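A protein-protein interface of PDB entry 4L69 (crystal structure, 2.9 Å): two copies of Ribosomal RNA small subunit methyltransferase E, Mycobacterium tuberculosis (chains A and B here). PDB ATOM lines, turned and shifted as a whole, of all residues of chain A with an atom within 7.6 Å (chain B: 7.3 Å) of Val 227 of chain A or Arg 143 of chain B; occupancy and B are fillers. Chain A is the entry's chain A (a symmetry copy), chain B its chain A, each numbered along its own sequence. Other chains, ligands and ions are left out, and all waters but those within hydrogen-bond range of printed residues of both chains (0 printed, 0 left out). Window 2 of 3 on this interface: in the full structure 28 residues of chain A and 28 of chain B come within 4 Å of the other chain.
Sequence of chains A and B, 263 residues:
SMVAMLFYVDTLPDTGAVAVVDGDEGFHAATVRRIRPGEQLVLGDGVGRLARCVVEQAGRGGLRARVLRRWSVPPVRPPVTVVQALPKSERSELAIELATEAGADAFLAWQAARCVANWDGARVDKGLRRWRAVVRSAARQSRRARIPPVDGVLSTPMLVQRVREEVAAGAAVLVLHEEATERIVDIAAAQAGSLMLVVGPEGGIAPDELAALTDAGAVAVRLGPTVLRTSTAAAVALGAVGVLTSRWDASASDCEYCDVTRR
Among the printed residues, pairs that only touch across the chains: Val 227 of chain A with Ser 142 of chain B (3.3 Å), Thr 226 of chain A with Ala 102 of chain B (3.5 Å), Arg 229 of chain A with Ser 142 of chain B (3.6 Å), Arg 229 of chain A with Ala 138 of chain B (3.8 Å), Thr 226 of chain A with Glu 101 of chain B (3.8 Å), Val 227 of chain A with Arg 143 of chain B (3.96 Å) and Thr 226 of chain A with Gly 103 of chain B (3.96 Å).
Of the printed residues of chain B, Glu 178 of chain A touches Arg 143. Of the printed residues of chain B, Thr 226 of chain A touches Glu 101 (3.8 Å), Ala 102 (3.5 Å) and Gly 103 (3.96 Å). Val 227 of chain A touches just these residues of chain B: Ser 142 (3.3 Å) and Arg 143 (3.96 Å). Leu 228 of chain A touches none of the printed residues of chain B. Of the printed residues of chain B, Arg 229 of chain A touches Glu 101, Ala 138, Gln 141 and Ser 142. Printed residues of chain A within 4 Å of Ala 102 of chain B: Thr 226 (3.5 Å). Of the printed residues of chain A, Gly 103 of chain B touches Thr 226. Arg 143 of chain B touches just these residues of chain A: Glu 178 and Val 227. Arg 144 of chain B touches none of the printed residues of chain A. The nearest printed residue of chain B that does not touch Val 227 of chain A is Glu 101 of chain B (4.4 Å). The nearest residue of chain A that does not touch Arg 143 of chain B is Arg 229 of chain A (6.3 Å). The nearest printed residue of chain A that does not touch Ala 138 of chain B is Val 227 of chain A (7.7 Å).
OE1 of Glu 178 of chain A lies within hydrogen-bond range of N of Leu 228 of chain A (3.3 Å). OG of Ser 142 of chain B lies within hydrogen-bond range of O of Ala 138 of chain B (3.1 Å). The backbone carbonyl oxygen (O) of Ser 137 of chain B sits close to the side-chain amide oxygen (OE1) of Gln 141 of chain B (3.1 Å). The side-chain hydroxyl of Thr 226 of chain A sits at hydrogen-bond distance from the backbone carbonyl oxygen of Leu 223 of chain A (2.6 Å).
Of the 11 printed residues of chain A, 5 touch a printed residue of chain B. Printed residues of chain A that touch a printed residue of chain B: Glu 178, Thr 226, Val 227, Arg 229 and Thr 232. Hydrophobic or aromatic side chains of chain A that line the printed part of chain B: Val 227. Along chain A the printed residues that touch a printed residue of chain B span positions 178 to 232. Printed residues of chain B that touch a printed residue of chain A: Glu 101, Ala 102, Gly 103, Ala 138, Gln 141, Ser 142 and Arg 143. Among the printed residues, 11 pairs touch across the chains. Among the printed residues, Asp or Glu carboxylates within 4 Å of a Lys or Arg side-chain nitrogen of the other chain: Glu 178 of chain A with Arg 143 of chain B and Arg 229 of chain A with Glu 101 of chain B.
The side-chain carboxylate (OE2) of Glu 178 of chain A is in salt-bridge range of the guanidinium group (NH2) of Arg 143 of chain B (3.8 Å). NH2 of Arg 229 of chain A lies close to NE2 of Gln 141 of chain B. OE2 of Glu 101 of chain B lies within salt-bridge range of NH1 of Arg 229 of chain A, at 3.4 Å. OG1 of Thr 232 of chain A is in hydrogen-bond range of OE1 of Glu 101 of chain B, at 2.6 Å.
No position is printed for both chains.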
ATOM      1  N   GLU A 178     -17.379  33.252  15.168  1.00  0.00           N
ATOM      2  CA  GLU A 178     -17.898  31.895  14.988  1.00  0.00           C
ATOM      3  C   GLU A 178     -18.234  31.555  13.542  1.00  0.00           C
ATOM      4  O   GLU A 178     -17.726  30.558  13.023  1.00  0.00           O
ATOM      5  CB  GLU A 178     -19.119  31.675  15.885  1.00  0.00           C
ATOM      6  CG  GLU A 178     -18.770  31.544  17.353  1.00  0.00           C
ATOM      7  CD  GLU A 178     -18.686  30.105  17.799  1.00  0.00           C
ATOM      8  OE1 GLU A 178     -17.698  29.420  17.447  1.00  0.00           O
ATOM      9  OE2 GLU A 178     -19.649  29.645  18.452  1.00  0.00           O
ATOM     10  N   LEU A 223     -11.803  29.683  15.350  1.00  0.00           N
ATOM     11  CA  LEU A 223     -10.899  28.831  16.126  1.00  0.00           C
ATOM     12  C   LEU A 223     -11.411  27.398  16.107  1.00  0.00           C
ATOM     13  O   LEU A 223     -11.838  26.866  17.132  1.00  0.00           O
ATOM     14  CB  LEU A 223     -10.726  29.322  17.577  1.00  0.00           C
ATOM     15  CG  LEU A 223      -9.982  30.623  17.823  1.00  0.00           C
ATOM     16  CD1 LEU A 223      -9.986  30.948  19.298  1.00  0.00           C
ATOM     17  CD2 LEU A 223      -8.545  30.548  17.345  1.00  0.00           C
ATOM     18  N   GLY A 224     -11.383  26.792  14.931  1.00  0.00           N
ATOM     19  CA  GLY A 224     -11.830  25.420  14.740  1.00  0.00           C
ATOM     20  C   GLY A 224     -13.300  25.188  15.051  1.00  0.00           C
ATOM     21  O   GLY A 224     -14.089  26.144  15.065  1.00  0.00           O
ATOM     22  N   PRO A 225     -13.699  23.914  15.323  1.00  0.00           N
ATOM     23  CA  PRO A 225     -15.118  23.632  15.614  1.00  0.00           C
ATOM     24  C   PRO A 225     -15.574  24.149  16.974  1.00  0.00           C
ATOM     25  O   PRO A 225     -16.778  24.243  17.224  1.00  0.00           O
ATOM     26  CB  PRO A 225     -15.215  22.098  15.524  1.00  0.00           C
ATOM     27  CG  PRO A 225     -13.890  21.620  15.015  1.00  0.00           C
ATOM     28  CD  PRO A 225     -12.896  22.676  15.364  1.00  0.00           C
ATOM     29  N   THR A 226     -14.606  24.493  17.838  1.00  0.00           N
ATOM     30  CA  THR A 226     -14.807  24.998  19.194  1.00  0.00           C
ATOM     31  C   THR A 226     -15.666  26.272  19.208  1.00  0.00           C
ATOM     32  O   THR A 226     -15.355  27.234  18.496  1.00  0.00           O
ATOM     33  CB  THR A 226     -13.443  25.152  19.954  1.00  0.00           C
ATOM     34  OG1 THR A 226     -12.732  26.321  19.529  1.00  0.00           O
ATOM     35  CG2 THR A 226     -12.543  23.914  19.844  1.00  0.00           C
ATOM     36  N   VAL A 227     -16.768  26.253  19.990  1.00  0.00           N
ATOM     37  CA  VAL A 227     -17.647  27.414  20.171  1.00  0.00           C
ATOM     38  C   VAL A 227     -16.880  28.407  21.066  1.00  0.00           C
ATOM     39  O   VAL A 227     -16.436  28.050  22.169  1.00  0.00           O
ATOM     40  CB  VAL A 227     -19.052  27.030  20.719  1.00  0.00           C
ATOM     41  CG1 VAL A 227     -19.770  28.221  21.347  1.00  0.00           C
ATOM     42  CG2 VAL A 227     -19.910  26.397  19.630  1.00  0.00           C
ATOM     43  N   LEU A 228     -16.667  29.625  20.537  1.00  0.00           N
ATOM     44  CA  LEU A 228     -15.919  30.703  21.190  1.00  0.00           C
ATOM     45  C   LEU A 228     -16.616  31.172  22.457  1.00  0.00           C
ATOM     46  O   LEU A 228     -17.742  31.667  22.402  1.00  0.00           O
ATOM     47  CB  LEU A 228     -15.673  31.889  20.227  1.00  0.00           C
ATOM     48  CG  LEU A 228     -15.208  31.570  18.796  1.00  0.00           C
ATOM     49  CD1 LEU A 228     -15.247  32.804  17.943  1.00  0.00           C
ATOM     50  CD2 LEU A 228     -13.810  30.970  18.771  1.00  0.00           C
ATOM     51  N   ARG A 229     -15.957  30.975  23.596  1.00  0.00           N
ATOM     52  CA  ARG A 229     -16.473  31.347  24.906  1.00  0.00           C
ATOM     53  C   ARG A 229     -15.662  32.528  25.425  1.00  0.00           C
ATOM     54  O   ARG A 229     -14.433  32.486  25.363  1.00  0.00           O
ATOM     55  CB  ARG A 229     -16.376  30.146  25.852  1.00  0.00           C
ATOM     56  CG  ARG A 229     -17.115  28.892  25.357  1.00  0.00           C
ATOM     57  CD  ARG A 229     -18.621  28.907  25.607  1.00  0.00           C
ATOM     58  NE  ARG A 229     -18.963  29.522  26.893  1.00  0.00           N
ATOM     59  CZ  ARG A 229     -18.990  28.884  28.059  1.00  0.00           C
ATOM     60  NH1 ARG A 229     -18.716  27.585  28.121  1.00  0.00           N
ATOM     61  NH2 ARG A 229     -19.298  29.538  29.171  1.00  0.00           N
ATOM     62  N   THR A 230     -16.341  33.598  25.900  1.00  0.00           N
ATOM     63  CA  THR A 230     -15.696  34.844  26.365  1.00  0.00           C
ATOM     64  C   THR A 230     -14.525  34.668  27.333  1.00  0.00           C
ATOM     65  O   THR A 230     -13.548  35.408  27.254  1.00  0.00           O
ATOM     66  CB  THR A 230     -16.716  35.884  26.814  1.00  0.00           C
ATOM     67  OG1 THR A 230     -17.463  35.350  27.901  1.00  0.00           O
ATOM     68  CG2 THR A 230     -17.651  36.315  25.685  1.00  0.00           C
ATOM     69  N   THR A 232     -12.473  31.772  27.533  1.00  0.00           N
ATOM     70  CA  THR A 232     -11.387  31.048  26.851  1.00  0.00           C
ATOM     71  C   THR A 232     -10.906  31.544  25.481  1.00  0.00           C
ATOM     72  O   THR A 232      -9.814  31.148  25.055  1.00  0.00           O
ATOM     73  CB  THR A 232     -11.712  29.555  26.739  1.00  0.00           C
ATOM     74  OG1 THR A 232     -13.089  29.387  26.419  1.00  0.00           O
ATOM     75  CG2 THR A 232     -11.349  28.786  27.977  1.00  0.00           C
ATOM     76  N   ALA A 233     -11.715  32.332  24.766  1.00  0.00           N
ATOM     77  CA  ALA A 233     -11.396  32.793  23.413  1.00  0.00           C
ATOM     78  C   ALA A 233      -9.974  33.331  23.196  1.00  0.00           C
ATOM     79  O   ALA A 233      -9.276  32.827  22.313  1.00  0.00           O
ATOM     80  CB  ALA A 233     -12.439  33.779  22.926  1.00  0.00           C
ATOM     81  N   VAL B   3     -29.180  32.851  19.151  1.00  0.00           N
ATOM     82  CA  VAL B   3     -28.627  31.503  18.979  1.00  0.00           C
ATOM     83  C   VAL B   3     -29.331  30.514  19.921  1.00  0.00           C
ATOM     84  O   VAL B   3     -29.509  30.810  21.108  1.00  0.00           O
ATOM     85  CB  VAL B   3     -27.074  31.444  19.113  1.00  0.00           C
ATOM     86  CG1 VAL B   3     -26.537  30.062  18.738  1.00  0.00           C
ATOM     87  CG2 VAL B   3     -26.399  32.519  18.262  1.00  0.00           C
ATOM     88  N   ALA B   4     -29.723  29.341  19.379  1.00  0.00           N
ATOM     89  CA  ALA B   4     -30.432  28.275  20.089  1.00  0.00           C
ATOM     90  C   ALA B   4     -29.610  27.632  21.203  1.00  0.00           C
ATOM     91  O   ALA B   4     -28.400  27.417  21.050  1.00  0.00           O
ATOM     92  CB  ALA B   4     -30.899  27.215  19.107  1.00  0.00           C
ATOM     93  N   MET B   5     -30.288  27.323  22.323  1.00  0.00           N
ATOM     94  CA  MET B   5     -29.681  26.697  23.494  1.00  0.00           C
ATOM     95  C   MET B   5     -29.737  25.186  23.408  1.00  0.00           C
ATOM     96  O   MET B   5     -30.755  24.614  23.006  1.00  0.00           O
ATOM     97  CB  MET B   5     -30.339  27.174  24.796  1.00  0.00           C
ATOM     98  CG  MET B   5     -29.944  28.578  25.193  1.00  0.00           C
ATOM     99  SD  MET B   5     -30.501  29.000  26.861  1.00  0.00           S
ATOM    100  CE  MET B   5     -29.080  28.486  27.800  1.00  0.00           C
ATOM    101  N   LEU B   6     -28.623  24.549  23.790  1.00  0.00           N
ATOM    102  CA  LEU B   6     -28.470  23.103  23.805  1.00  0.00           C
ATOM    103  C   LEU B   6     -28.920  22.544  25.144  1.00  0.00           C
ATOM    104  O   LEU B   6     -28.633  23.133  26.188  1.00  0.00           O
ATOM    105  CB  LEU B   6     -27.009  22.702  23.516  1.00  0.00           C
ATOM    106  CG  LEU B   6     -26.713  21.201  23.437  1.00  0.00           C
ATOM    107  CD1 LEU B   6     -27.298  20.583  22.187  1.00  0.00           C
ATOM    108  CD2 LEU B   6     -25.246  20.940  23.489  1.00  0.00           C
ATOM    109  N   TYR B   8     -29.109  18.624  27.114  1.00  0.00           N
ATOM    110  CA  TYR B   8     -28.806  17.199  27.065  1.00  0.00           C
ATOM    111  C   TYR B   8     -29.946  16.341  27.601  1.00  0.00           C
ATOM    112  O   TYR B   8     -30.529  16.639  28.649  1.00  0.00           O
ATOM    113  CB  TYR B   8     -27.476  16.850  27.743  1.00  0.00           C
ATOM    114  CG  TYR B   8     -26.247  17.474  27.127  1.00  0.00           C
ATOM    115  CD1 TYR B   8     -25.916  17.242  25.791  1.00  0.00           C
ATOM    116  CD2 TYR B   8     -25.358  18.218  27.900  1.00  0.00           C
ATOM    117  CE1 TYR B   8     -24.762  17.785  25.226  1.00  0.00           C
ATOM    118  CE2 TYR B   8     -24.194  18.755  27.349  1.00  0.00           C
ATOM    119  CZ  TYR B   8     -23.903  18.537  26.010  1.00  0.00           C
ATOM    120  OH  TYR B   8     -22.756  19.052  25.473  1.00  0.00           O
ATOM    121  N   VAL B  42     -32.015  23.308  20.512  1.00  0.00           N
ATOM    122  CA  VAL B  42     -31.298  22.111  20.067  1.00  0.00           C
ATOM    123  C   VAL B  42     -31.234  21.127  21.234  1.00  0.00           C
ATOM    124  O   VAL B  42     -30.946  21.531  22.355  1.00  0.00           O
ATOM    125  CB  VAL B  42     -29.885  22.402  19.469  1.00  0.00           C
ATOM    126  CG1 VAL B  42     -29.284  21.154  18.829  1.00  0.00           C
ATOM    127  CG2 VAL B  42     -29.923  23.540  18.453  1.00  0.00           C
ATOM    128  N   LEU B  50     -27.582  15.119  17.754  1.00  0.00           N
ATOM    129  CA  LEU B  50     -28.230  16.423  17.948  1.00  0.00           C
ATOM    130  C   LEU B  50     -29.569  16.481  17.227  1.00  0.00           C
ATOM    131  O   LEU B  50     -29.728  15.899  16.156  1.00  0.00           O
ATOM    132  CB  LEU B  50     -27.338  17.592  17.467  1.00  0.00           C
ATOM    133  CG  LEU B  50     -25.971  17.771  18.144  1.00  0.00           C
ATOM    134  CD1 LEU B  50     -25.093  18.712  17.356  1.00  0.00           C
ATOM    135  CD2 LEU B  50     -26.102  18.261  19.578  1.00  0.00           C
ATOM    136  N   ARG B  52     -32.784  19.404  16.204  1.00  0.00           N
ATOM    137  CA  ARG B  52     -33.332  20.759  16.149  1.00  0.00           C
ATOM    138  C   ARG B  52     -34.809  20.638  16.540  1.00  0.00           C
ATOM    139  O   ARG B  52     -35.544  19.890  15.893  1.00  0.00           O
ATOM    140  CB  ARG B  52     -33.167  21.350  14.736  1.00  0.00           C
ATOM    141  CG  ARG B  52     -33.421  22.850  14.643  1.00  0.00           C
ATOM    142  CD  ARG B  52     -32.208  23.675  15.028  1.00  0.00           C
ATOM    143  NE  ARG B  52     -32.570  25.077  15.229  1.00  0.00           N
ATOM    144  CZ  ARG B  52     -31.711  26.044  15.530  1.00  0.00           C
ATOM    145  NH1 ARG B  52     -30.417  25.775  15.667  1.00  0.00           N
ATOM    146  NH2 ARG B  52     -32.135  27.290  15.691  1.00  0.00           N
ATOM    147  N   THR B 100     -12.620  21.906  28.326  1.00  0.00           N
ATOM    148  CA  THR B 100     -13.866  21.464  27.675  1.00  0.00           C
ATOM    149  C   THR B 100     -14.267  22.496  26.636  1.00  0.00           C
ATOM    150  O   THR B 100     -14.571  22.121  25.502  1.00  0.00           O
ATOM    151  CB  THR B 100     -14.975  21.159  28.697  1.00  0.00           C
ATOM    152  OG1 THR B 100     -14.487  20.237  29.673  1.00  0.00           O
ATOM    153  CG2 THR B 100     -16.226  20.576  28.046  1.00  0.00           C
ATOM    154  N   GLU B 101     -14.220  23.793  27.003  1.00  0.00           N
ATOM    155  CA  GLU B 101     -14.514  24.884  26.071  1.00  0.00           C
ATOM    156  C   GLU B 101     -13.490  24.840  24.914  1.00  0.00           C
ATOM    157  O   GLU B 101     -13.889  24.860  23.744  1.00  0.00           O
ATOM    158  CB  GLU B 101     -14.473  26.248  26.777  1.00  0.00           C
ATOM    159  CG  GLU B 101     -15.575  26.469  27.795  1.00  0.00           C
ATOM    160  CD  GLU B 101     -15.372  27.642  28.737  1.00  0.00           C
ATOM    161  OE1 GLU B 101     -14.766  28.657  28.320  1.00  0.00           O
ATOM    162  OE2 GLU B 101     -15.845  27.555  29.892  1.00  0.00           O
ATOM    163  N   ALA B 102     -12.184  24.671  25.255  1.00  0.00           N
ATOM    164  CA  ALA B 102     -11.060  24.583  24.311  1.00  0.00           C
ATOM    165  C   ALA B 102     -11.104  23.370  23.372  1.00  0.00           C
ATOM    166  O   ALA B 102     -10.289  23.293  22.452  1.00  0.00           O
ATOM    167  CB  ALA B 102      -9.740  24.613  25.066  1.00  0.00           C
ATOM    168  N   GLY B 103     -12.017  22.430  23.617  1.00  0.00           N
ATOM    169  CA  GLY B 103     -12.191  21.260  22.765  1.00  0.00           C
ATOM    170  C   GLY B 103     -11.523  19.955  23.147  1.00  0.00           C
ATOM    171  O   GLY B 103     -11.307  19.122  22.263  1.00  0.00           O
ATOM    172  N   SER B 137     -21.767  20.688  32.067  1.00  0.00           N
ATOM    173  CA  SER B 137     -22.181  22.086  32.042  1.00  0.00           C
ATOM    174  C   SER B 137     -21.390  22.901  31.020  1.00  0.00           C
ATOM    175  O   SER B 137     -22.002  23.624  30.230  1.00  0.00           O
ATOM    176  CB  SER B 137     -22.073  22.703  33.429  1.00  0.00           C
ATOM    177  OG  SER B 137     -22.624  24.007  33.407  1.00  0.00           O
ATOM    178  N   ALA B 138     -20.040  22.764  31.017  1.00  0.00           N
ATOM    179  CA  ALA B 138     -19.165  23.474  30.077  1.00  0.00           C
ATOM    180  C   ALA B 138     -19.459  23.038  28.649  1.00  0.00           C
ATOM    181  O   ALA B 138     -19.587  23.897  27.781  1.00  0.00           O
ATOM    182  CB  ALA B 138     -17.699  23.241  30.423  1.00  0.00           C
ATOM    183  N   ALA B 139     -19.655  21.718  28.435  1.00  0.00           N
ATOM    184  CA  ALA B 139     -19.972  21.096  27.151  1.00  0.00           C
ATOM    185  C   ALA B 139     -21.290  21.628  26.597  1.00  0.00           C
ATOM    186  O   ALA B 139     -21.385  21.891  25.395  1.00  0.00           O
ATOM    187  CB  ALA B 139     -20.039  19.586  27.307  1.00  0.00           C
ATOM    188  N   ARG B 140     -22.292  21.821  27.484  1.00  0.00           N
ATOM    189  CA  ARG B 140     -23.619  22.326  27.150  1.00  0.00           C
ATOM    190  C   ARG B 140     -23.509  23.749  26.645  1.00  0.00           C
ATOM    191  O   ARG B 140     -24.051  24.056  25.585  1.00  0.00           O
ATOM    192  CB  ARG B 140     -24.533  22.262  28.383  1.00  0.00           C
ATOM    193  CG  ARG B 140     -26.009  22.447  28.063  1.00  0.00           C
ATOM    194  CD  ARG B 140     -26.823  22.924  29.256  1.00  0.00           C
ATOM    195  NE  ARG B 140     -26.504  24.300  29.648  1.00  0.00           N
ATOM    196  CZ  ARG B 140     -27.075  25.386  29.133  1.00  0.00           C
ATOM    197  NH1 ARG B 140     -27.997  25.275  28.184  1.00  0.00           N
ATOM    198  NH2 ARG B 140     -26.719  26.593  29.555  1.00  0.00           N
ATOM    199  N   GLN B 141     -22.786  24.609  27.390  1.00  0.00           N
ATOM    200  CA  GLN B 141     -22.571  26.015  27.046  1.00  0.00           C
ATOM    201  C   GLN B 141     -21.705  26.164  25.800  1.00  0.00           C
ATOM    202  O   GLN B 141     -21.880  27.121  25.051  1.00  0.00           O
ATOM    203  CB  GLN B 141     -21.992  26.786  28.232  1.00  0.00           C
ATOM    204  CG  GLN B 141     -22.992  26.974  29.379  1.00  0.00           C
ATOM    205  CD  GLN B 141     -22.315  27.296  30.690  1.00  0.00           C
ATOM    206  OE1 GLN B 141     -22.025  26.411  31.503  1.00  0.00           O
ATOM    207  NE2 GLN B 141     -22.054  28.575  30.927  1.00  0.00           N
ATOM    208  N   SER B 142     -20.831  25.174  25.539  1.00  0.00           N
ATOM    209  CA  SER B 142     -19.969  25.125  24.349  1.00  0.00           C
ATOM    210  C   SER B 142     -20.684  24.446  23.178  1.00  0.00           C
ATOM    211  O   SER B 142     -20.046  24.175  22.158  1.00  0.00           O
ATOM    212  CB  SER B 142     -18.667  24.393  24.659  1.00  0.00           C
ATOM    213  OG  SER B 142     -17.867  25.155  25.546  1.00  0.00           O
ATOM    214  N   ARG B 143     -22.009  24.162  23.332  1.00  0.00           N
ATOM    215  CA  ARG B 143     -22.875  23.497  22.345  1.00  0.00           C
ATOM    216  C   ARG B 143     -22.245  22.207  21.754  1.00  0.00           C
ATOM    217  O   ARG B 143     -22.327  21.965  20.548  1.00  0.00           O
ATOM    218  CB  ARG B 143     -23.339  24.483  21.252  1.00  0.00           C
ATOM    219  CG  ARG B 143     -24.220  25.615  21.779  1.00  0.00           C
ATOM    220  CD  ARG B 143     -25.132  26.235  20.726  1.00  0.00           C
ATOM    221  NE  ARG B 143     -24.404  26.683  19.533  1.00  0.00           N
ATOM    222  CZ  ARG B 143     -23.814  27.870  19.403  1.00  0.00           C
ATOM    223  NH1 ARG B 143     -23.858  28.754  20.394  1.00  0.00           N
ATOM    224  NH2 ARG B 143     -23.179  28.183  18.282  1.00  0.00           N
ATOM    225  N   ARG B 144     -21.608  21.390  22.620  1.00  0.00           N
ATOM    226  CA  ARG B 144     -20.900  20.160  22.250  1.00  0.00           C
ATOM    227  C   ARG B 144     -21.792  18.943  22.042  1.00  0.00           C
ATOM    228  O   ARG B 144     -22.587  18.594  22.913  1.00  0.00           O
ATOM    229  CB  ARG B 144     -19.781  19.834  23.254  1.00  0.00           C
ATOM    230  CG  ARG B 144     -18.637  20.847  23.266  1.00  0.00           C
ATOM    231  CD  ARG B 144     -17.422  20.379  24.057  1.00  0.00           C
ATOM    232  NE  ARG B 144     -16.795  19.196  23.463  1.00  0.00           N
ATOM    233  CZ  ARG B 144     -15.547  18.810  23.695  1.00  0.00           C
ATOM    234  NH1 ARG B 144     -14.766  19.514  24.504  1.00  0.00           N
ATOM    235  NH2 ARG B 144     -15.065  17.723  23.113  1.00  0.00           N
ATOM    236  N   ALA B 145     -21.626  18.274  20.897  1.00  0.00           N
ATOM    237  CA  ALA B 145     -22.355  17.056  20.555  1.00  0.00           C
ATOM    238  C   ALA B 145     -21.895  15.890  21.449  1.00  0.00           C
ATOM    239  O   ALA B 145     -22.711  15.063  21.845  1.00  0.00           O
ATOM    240  CB  ALA B 145     -22.120  16.715  19.102  1.00  0.00           C
ATOM    241  N   ARG B 146     -20.592  15.839  21.762  1.00  0.00           N
ATOM    242  CA  ARG B 146     -19.989  14.808  22.608  1.00  0.00           C
ATOM    243  C   ARG B 146     -19.418  15.411  23.887  1.00  0.00           C
ATOM    244  O   ARG B 146     -18.539  16.283  23.834  1.00  0.00           O
ATOM    245  CB  ARG B 146     -18.892  14.036  21.851  1.00  0.00           C
ATOM    246  CG  ARG B 146     -19.434  13.296  20.660  1.00  0.00           C
ATOM    247  CD  ARG B 146     -18.366  12.719  19.772  1.00  0.00           C
ATOM    248  NE  ARG B 146     -18.978  12.083  18.606  1.00  0.00           N
ATOM    249  CZ  ARG B 146     -19.419  10.831  18.580  1.00  0.00           C
ATOM    250  NH1 ARG B 146     -19.303  10.055  19.652  1.00  0.00           N
ATOM    251  NH2 ARG B 146     -19.974  10.341  17.480  1.00  0.00           N
